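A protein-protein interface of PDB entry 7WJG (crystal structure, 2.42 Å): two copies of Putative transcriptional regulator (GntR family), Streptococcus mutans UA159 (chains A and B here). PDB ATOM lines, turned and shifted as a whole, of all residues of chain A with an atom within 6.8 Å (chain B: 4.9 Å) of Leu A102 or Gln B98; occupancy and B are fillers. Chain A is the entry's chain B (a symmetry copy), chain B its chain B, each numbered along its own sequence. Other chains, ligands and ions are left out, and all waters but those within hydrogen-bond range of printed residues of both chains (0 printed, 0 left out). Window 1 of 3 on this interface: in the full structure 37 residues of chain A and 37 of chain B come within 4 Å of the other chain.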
ATOM      1  N   LYS A  97      27.416  30.613 -16.545  1.00  0.00           N
ATOM      2  CA  LYS A  97      26.120  29.982 -16.758  1.00  0.00           C
ATOM      3  C   LYS A  97      25.795  29.030 -15.612  1.00  0.00           C
ATOM      4  O   LYS A  97      24.702  29.080 -15.032  1.00  0.00           O
ATOM      5  CB  LYS A  97      26.145  29.255 -18.111  1.00  0.00           C
ATOM      6  CG  LYS A  97      24.927  28.419 -18.511  1.00  0.00           C
ATOM      7  CD  LYS A  97      23.583  28.958 -18.008  1.00  0.00           C
ATOM      8  CE  LYS A  97      22.471  27.923 -18.212  1.00  0.00           C
ATOM      9  NZ  LYS A  97      22.482  26.842 -17.174  1.00  0.00           N
ATOM     10  N   GLN A  98      26.744  28.167 -15.250  1.00  0.00           N
ATOM     11  CA  GLN A  98      26.472  27.209 -14.185  1.00  0.00           C
ATOM     12  C   GLN A  98      26.225  27.893 -12.846  1.00  0.00           C
ATOM     13  O   GLN A  98      25.327  27.491 -12.096  1.00  0.00           O
ATOM     14  CB  GLN A  98      27.616  26.204 -14.101  1.00  0.00           C
ATOM     15  CG  GLN A  98      27.302  24.976 -14.957  1.00  0.00           C
ATOM     16  CD  GLN A  98      27.782  23.683 -14.336  1.00  0.00           C
ATOM     17  OE1 GLN A  98      27.002  22.710 -14.168  1.00  0.00           O
ATOM     18  NE2 GLN A  98      29.086  23.656 -13.992  1.00  0.00           N
ATOM     19  N   LYS A  99      26.997  28.928 -12.531  1.00  0.00           N
ATOM     20  CA  LYS A  99      26.733  29.687 -11.314  1.00  0.00           C
ATOM     21  C   LYS A  99      25.306  30.229 -11.302  1.00  0.00           C
ATOM     22  O   LYS A  99      24.607  30.158 -10.286  1.00  0.00           O
ATOM     23  CB  LYS A  99      27.738  30.830 -11.178  1.00  0.00           C
ATOM     24  CG  LYS A  99      27.434  31.795 -10.033  1.00  0.00           C
ATOM     25  CD  LYS A  99      27.902  33.220 -10.328  1.00  0.00           C
ATOM     26  CE  LYS A  99      28.666  33.829  -9.148  1.00  0.00           C
ATOM     27  NZ  LYS A  99      27.910  33.728  -7.863  1.00  0.00           N
ATOM     28  N   GLN A 100      24.864  30.789 -12.424  1.00  0.00           N
ATOM     29  CA  GLN A 100      23.503  31.306 -12.506  1.00  0.00           C
ATOM     30  C   GLN A 100      22.485  30.188 -12.343  1.00  0.00           C
ATOM     31  O   GLN A 100      21.485  30.339 -11.634  1.00  0.00           O
ATOM     32  CB  GLN A 100      23.300  32.017 -13.839  1.00  0.00           C
ATOM     33  CG  GLN A 100      24.020  33.332 -13.936  1.00  0.00           C
ATOM     34  CD  GLN A 100      24.228  33.762 -15.369  1.00  0.00           C
ATOM     35  OE1 GLN A 100      23.987  32.992 -16.307  1.00  0.00           O
ATOM     36  NE2 GLN A 100      24.676  35.001 -15.551  1.00  0.00           N
ATOM     37  N   GLU A 101      22.729  29.056 -13.004  1.00  0.00           N
ATOM     38  CA  GLU A 101      21.810  27.928 -12.939  1.00  0.00           C
ATOM     39  C   GLU A 101      21.709  27.379 -11.520  1.00  0.00           C
ATOM     40  O   GLU A 101      20.613  27.071 -11.033  1.00  0.00           O
ATOM     41  CB  GLU A 101      22.279  26.845 -13.915  1.00  0.00           C
ATOM     42  CG  GLU A 101      21.256  25.791 -14.290  1.00  0.00           C
ATOM     43  CD  GLU A 101      20.097  26.333 -15.132  1.00  0.00           C
ATOM     44  OE1 GLU A 101      20.218  27.452 -15.703  1.00  0.00           O
ATOM     45  OE2 GLU A 101      19.061  25.630 -15.211  1.00  0.00           O
ATOM     46  N   LEU A 102      22.844  27.259 -10.836  1.00  0.00           N
ATOM     47  CA  LEU A 102      22.813  26.760  -9.472  1.00  0.00           C
ATOM     48  C   LEU A 102      22.088  27.731  -8.545  1.00  0.00           C
ATOM     49  O   LEU A 102      21.326  27.311  -7.666  1.00  0.00           O
ATOM     50  CB  LEU A 102      24.239  26.505  -8.988  1.00  0.00           C
ATOM     51  CG  LEU A 102      24.284  25.918  -7.584  1.00  0.00           C
ATOM     52  CD1 LEU A 102      24.994  24.557  -7.578  1.00  0.00           C
ATOM     53  CD2 LEU A 102      24.934  26.922  -6.634  1.00  0.00           C
ATOM     54  N   ASP A 103      22.304  29.035  -8.731  1.00  0.00           N
ATOM     55  CA  ASP A 103      21.557  30.021  -7.957  1.00  0.00           C
ATOM     56  C   ASP A 103      20.063  29.912  -8.225  1.00  0.00           C
ATOM     57  O   ASP A 103      19.248  29.964  -7.296  1.00  0.00           O
ATOM     58  CB  ASP A 103      22.057  31.427  -8.288  1.00  0.00           C
ATOM     59  CG  ASP A 103      21.193  32.526  -7.679  1.00  0.00           C
ATOM     60  OD1 ASP A 103      20.123  32.866  -8.246  1.00  0.00           O
ATOM     61  OD2 ASP A 103      21.598  33.055  -6.623  1.00  0.00           O
ATOM     62  N   ALA A 104      19.683  29.767  -9.493  1.00  0.00           N
ATOM     63  CA  ALA A 104      18.275  29.578  -9.812  1.00  0.00           C
ATOM     64  C   ALA A 104      17.728  28.344  -9.111  1.00  0.00           C
ATOM     65  O   ALA A 104      16.686  28.397  -8.446  1.00  0.00           O
ATOM     66  CB  ALA A 104      18.097  29.459 -11.321  1.00  0.00           C
ATOM     67  N   MET A 105      18.442  27.225  -9.237  1.00  0.00           N
ATOM     68  CA  MET A 105      18.035  25.984  -8.597  1.00  0.00           C
ATOM     69  C   MET A 105      17.866  26.163  -7.093  1.00  0.00           C
ATOM     70  O   MET A 105      16.976  25.560  -6.481  1.00  0.00           O
ATOM     71  CB  MET A 105      19.068  24.900  -8.891  1.00  0.00           C
ATOM     72  CG  MET A 105      19.084  23.781  -7.875  1.00  0.00           C
ATOM     73  SD  MET A 105      17.710  22.684  -8.226  1.00  0.00           S
ATOM     74  CE  MET A 105      18.308  21.994  -9.774  1.00  0.00           C
ATOM     75  N   ASN A 106      18.710  26.989  -6.480  1.00  0.00           N
ATOM     76  CA  ASN A 106      18.605  27.227  -5.049  1.00  0.00           C
ATOM     77  C   ASN A 106      17.219  27.735  -4.673  1.00  0.00           C
ATOM     78  O   ASN A 106      16.594  27.232  -3.732  1.00  0.00           O
ATOM     79  CB  ASN A 106      19.676  28.220  -4.620  1.00  0.00           C
ATOM     80  CG  ASN A 106      20.368  27.801  -3.358  1.00  0.00           C
ATOM     81  OD1 ASN A 106      19.745  27.667  -2.304  1.00  0.00           O
ATOM     82  ND2 ASN A 106      21.664  27.558  -3.460  1.00  0.00           N
ATOM     83  N   LYS A 107      16.717  28.729  -5.413  1.00  0.00           N
ATOM     84  CA  LYS A 107      15.393  29.278  -5.137  1.00  0.00           C
ATOM     85  C   LYS A 107      14.284  28.272  -5.449  1.00  0.00           C
ATOM     86  O   LYS A 107      13.342  28.127  -4.664  1.00  0.00           O
ATOM     87  CB  LYS A 107      15.196  30.574  -5.922  1.00  0.00           C
ATOM     88  CG  LYS A 107      16.081  31.710  -5.419  1.00  0.00           C
ATOM     89  CD  LYS A 107      16.485  32.699  -6.519  1.00  0.00           C
ATOM     90  CE  LYS A 107      15.350  33.687  -6.844  1.00  0.00           C
ATOM     91  NZ  LYS A 107      15.720  35.139  -6.640  1.00  0.00           N
ATOM     92  N   SER B  94      23.857  20.816   1.086  1.00  0.00           N
ATOM     93  CA  SER B  94      24.408  20.272  -0.146  1.00  0.00           C
ATOM     94  C   SER B  94      24.514  21.353  -1.213  1.00  0.00           C
ATOM     95  O   SER B  94      25.515  21.434  -1.934  1.00  0.00           O
ATOM     96  CB  SER B  94      23.544  19.111  -0.636  1.00  0.00           C
ATOM     97  OG  SER B  94      23.832  18.815  -1.996  1.00  0.00           O
ATOM     98  N   LEU B  95      23.502  22.214  -1.306  1.00  0.00           N
ATOM     99  CA  LEU B  95      23.530  23.296  -2.286  1.00  0.00           C
ATOM    100  C   LEU B  95      24.646  24.281  -1.981  1.00  0.00           C
ATOM    101  O   LEU B  95      25.294  24.804  -2.896  1.00  0.00           O
ATOM    102  CB  LEU B  95      22.181  24.022  -2.317  1.00  0.00           C
ATOM    103  CG  LEU B  95      21.081  23.264  -3.062  1.00  0.00           C
ATOM    104  CD1 LEU B  95      19.710  23.710  -2.600  1.00  0.00           C
ATOM    105  CD2 LEU B  95      21.229  23.452  -4.563  1.00  0.00           C
ATOM    106  N   LEU B  96      24.869  24.565  -0.697  1.00  0.00           N
ATOM    107  CA  LEU B  96      25.950  25.462  -0.311  1.00  0.00           C
ATOM    108  C   LEU B  96      27.312  24.837  -0.599  1.00  0.00           C
ATOM    109  O   LEU B  96      28.221  25.516  -1.087  1.00  0.00           O
ATOM    110  CB  LEU B  96      25.812  25.824   1.164  1.00  0.00           C
ATOM    111  CG  LEU B  96      26.916  26.749   1.686  1.00  0.00           C
ATOM    112  CD1 LEU B  96      26.677  28.196   1.226  1.00  0.00           C
ATOM    113  CD2 LEU B  96      27.048  26.655   3.211  1.00  0.00           C
ATOM    114  N   LYS B  97      27.458  23.538  -0.310  1.00  0.00           N
ATOM    115  CA  LYS B  97      28.646  22.789  -0.698  1.00  0.00           C
ATOM    116  C   LYS B  97      28.909  22.941  -2.192  1.00  0.00           C
ATOM    117  O   LYS B  97      30.030  23.255  -2.614  1.00  0.00           O
ATOM    118  CB  LYS B  97      28.450  21.317  -0.302  1.00  0.00           C
ATOM    119  CG  LYS B  97      29.523  20.305  -0.708  1.00  0.00           C
ATOM    120  CD  LYS B  97      30.952  20.859  -0.735  1.00  0.00           C
ATOM    121  CE  LYS B  97      31.906  19.868  -1.413  1.00  0.00           C
ATOM    122  NZ  LYS B  97      31.813  19.899  -2.909  1.00  0.00           N
ATOM    123  N   GLN B  98      27.877  22.749  -3.014  1.00  0.00           N
ATOM    124  CA  GLN B  98      28.082  22.844  -4.455  1.00  0.00           C
ATOM    125  C   GLN B  98      28.492  24.248  -4.884  1.00  0.00           C
ATOM    126  O   GLN B  98      29.371  24.407  -5.740  1.00  0.00           O
ATOM    127  CB  GLN B  98      26.823  22.380  -5.179  1.00  0.00           C
ATOM    128  CG  GLN B  98      26.925  20.889  -5.507  1.00  0.00           C
ATOM    129  CD  GLN B  98      26.316  20.534  -6.846  1.00  0.00           C
ATOM    130  OE1 GLN B  98      26.970  19.901  -7.713  1.00  0.00           O
ATOM    131  NE2 GLN B  98      25.042  20.937  -7.026  1.00  0.00           N
ATOM    132  N   LYS B  99      27.881  25.275  -4.302  1.00  0.00           N
ATOM    133  CA  LYS B  99      28.311  26.637  -4.594  1.00  0.00           C
ATOM    134  C   LYS B  99      29.795  26.824  -4.289  1.00  0.00           C
ATOM    135  O   LYS B  99      30.535  27.425  -5.074  1.00  0.00           O
ATOM    136  CB  LYS B  99      27.473  27.636  -3.797  1.00  0.00           C
ATOM    137  CG  LYS B  99      27.965  29.079  -3.893  1.00  0.00           C
ATOM    138  CD  LYS B  99      27.671  29.884  -2.627  1.00  0.00           C
ATOM    139  CE  LYS B  99      27.061  31.252  -2.945  1.00  0.00           C
ATOM    140  NZ  LYS B  99      27.870  32.022  -3.939  1.00  0.00           N
ATOM    141  N   GLN B 100      30.241  26.325  -3.140  1.00  0.00           N
ATOM    142  CA  GLN B 100      31.651  26.435  -2.785  1.00  0.00           C
ATOM    143  C   GLN B 100      32.522  25.669  -3.768  1.00  0.00           C
ATOM    144  O   GLN B 100      33.572  26.157  -4.200  1.00  0.00           O
ATOM    145  CB  GLN B 100      31.869  25.915  -1.368  1.00  0.00           C
ATOM    146  CG  GLN B 100      31.323  26.824  -0.303  1.00  0.00           C
ATOM    147  CD  GLN B 100      31.092  26.095   1.001  1.00  0.00           C
ATOM    148  OE1 GLN B 100      31.176  24.863   1.066  1.00  0.00           O
ATOM    149  NE2 GLN B 100      30.800  26.854   2.053  1.00  0.00           N
ATOM    150  N   GLU B 101      32.096  24.459  -4.128  1.00  0.00           N
ATOM    151  CA  GLU B 101      32.862  23.627  -5.047  1.00  0.00           C
ATOM    152  C   GLU B 101      32.970  24.278  -6.421  1.00  0.00           C
ATOM    153  O   GLU B 101      34.042  24.283  -7.040  1.00  0.00           O
ATOM    154  CB  GLU B 101      32.200  22.249  -5.142  1.00  0.00           C
ATOM    155  CG  GLU B 101      33.054  21.133  -5.713  1.00  0.00           C
ATOM    156  CD  GLU B 101      34.223  20.733  -4.809  1.00  0.00           C
ATOM    157  OE1 GLU B 101      34.218  21.085  -3.598  1.00  0.00           O
ATOM    158  OE2 GLU B 101      35.153  20.067  -5.326  1.00  0.00           O
ATOM    159  N   LEU B 102      31.870  24.844  -6.911  1.00  0.00           N
ATOM    160  CA  LEU B 102      31.913  25.499  -8.208  1.00  0.00           C
ATOM    161  C   LEU B 102      32.811  26.732  -8.174  1.00  0.00           C
ATOM    162  O   LEU B 102      33.559  26.990  -9.123  1.00  0.00           O
ATOM    163  CB  LEU B 102      30.496  25.865  -8.642  1.00  0.00           C
ATOM    164  CG  LEU B 102      30.454  26.500 -10.026  1.00  0.00           C
ATOM    165  CD1 LEU B 102      29.574  25.682 -10.981  1.00  0.00           C
ATOM    166  CD2 LEU B 102      29.997  27.952  -9.906  1.00  0.00           C
ATOM    167  N   ASP B 103      32.756  27.502  -7.085  1.00  0.00           N
ATOM    168  CA  ASP B 103      33.668  28.631  -6.937  1.00  0.00           C
ATOM    169  C   ASP B 103      35.118  28.168  -6.918  1.00  0.00           C
ATOM    170  O   ASP B 103      35.984  28.773  -7.562  1.00  0.00           O
ATOM    171  CB  ASP B 103      33.338  29.400  -5.658  1.00  0.00           C
ATOM    172  CG  ASP B 103      34.372  30.470  -5.322  1.00  0.00           C
ATOM    173  OD1 ASP B 103      35.443  30.146  -4.748  1.00  0.00           O
ATOM    174  OD2 ASP B 103      34.100  31.648  -5.635  1.00  0.00           O
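Among the printed residues, pairs that only touch across the chains: Gln A98 with Leu B102 (3.7 Å), Leu A102 with Gln B98 (3.7 Å), Asn A106 with Leu B95 (3.8 Å), Lys A99 with Leu B102 (3.9 Å), Leu A102 with Lys B99 (3.9 Å) and Met A105 with Leu B95 (3.96 Å).
Leu A102 touches two residues of chain B. Of the printed residues of chain A, Leu B95 touches Met A105 (3.96 Å) and Asn A106 (3.8 Å). Of the printed residues of chain B, Gln A98 touches Leu B102. Printed residues of chain A within 4 Å of Lys B99: Leu A102 (3.9 Å). Gln A100 touches none of the printed residues of chain B. Ser B94 touches none of the printed residues of chain A. The nearest printed residue of chain B that does not touch Lys A99 is Lys B99 (4.3 Å).
Of the 10 printed residues of chain B, 4 touch a printed residue of chain A. Hydrophobic or aromatic side chains of chain B within 4 Å of the printed part of chain A: Leu B95 and Leu B102. Hydrophobic or aromatic side chains of chain A that line the printed part of chain B: Leu A102 and Met A105. Among the printed residues, 6 pairs touch across the chains. Among the printed residues, no Asp or Glu carboxylate lies within 4 Å of a Lys or Arg side-chain nitrogen of the other chain.
Gln A98 touches Leu B102, and with the chains exchanged Leu A102 touches Gln B98. Lys A99 touches Leu B102, and with the chains exchanged Leu A102 touches Lys B99.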
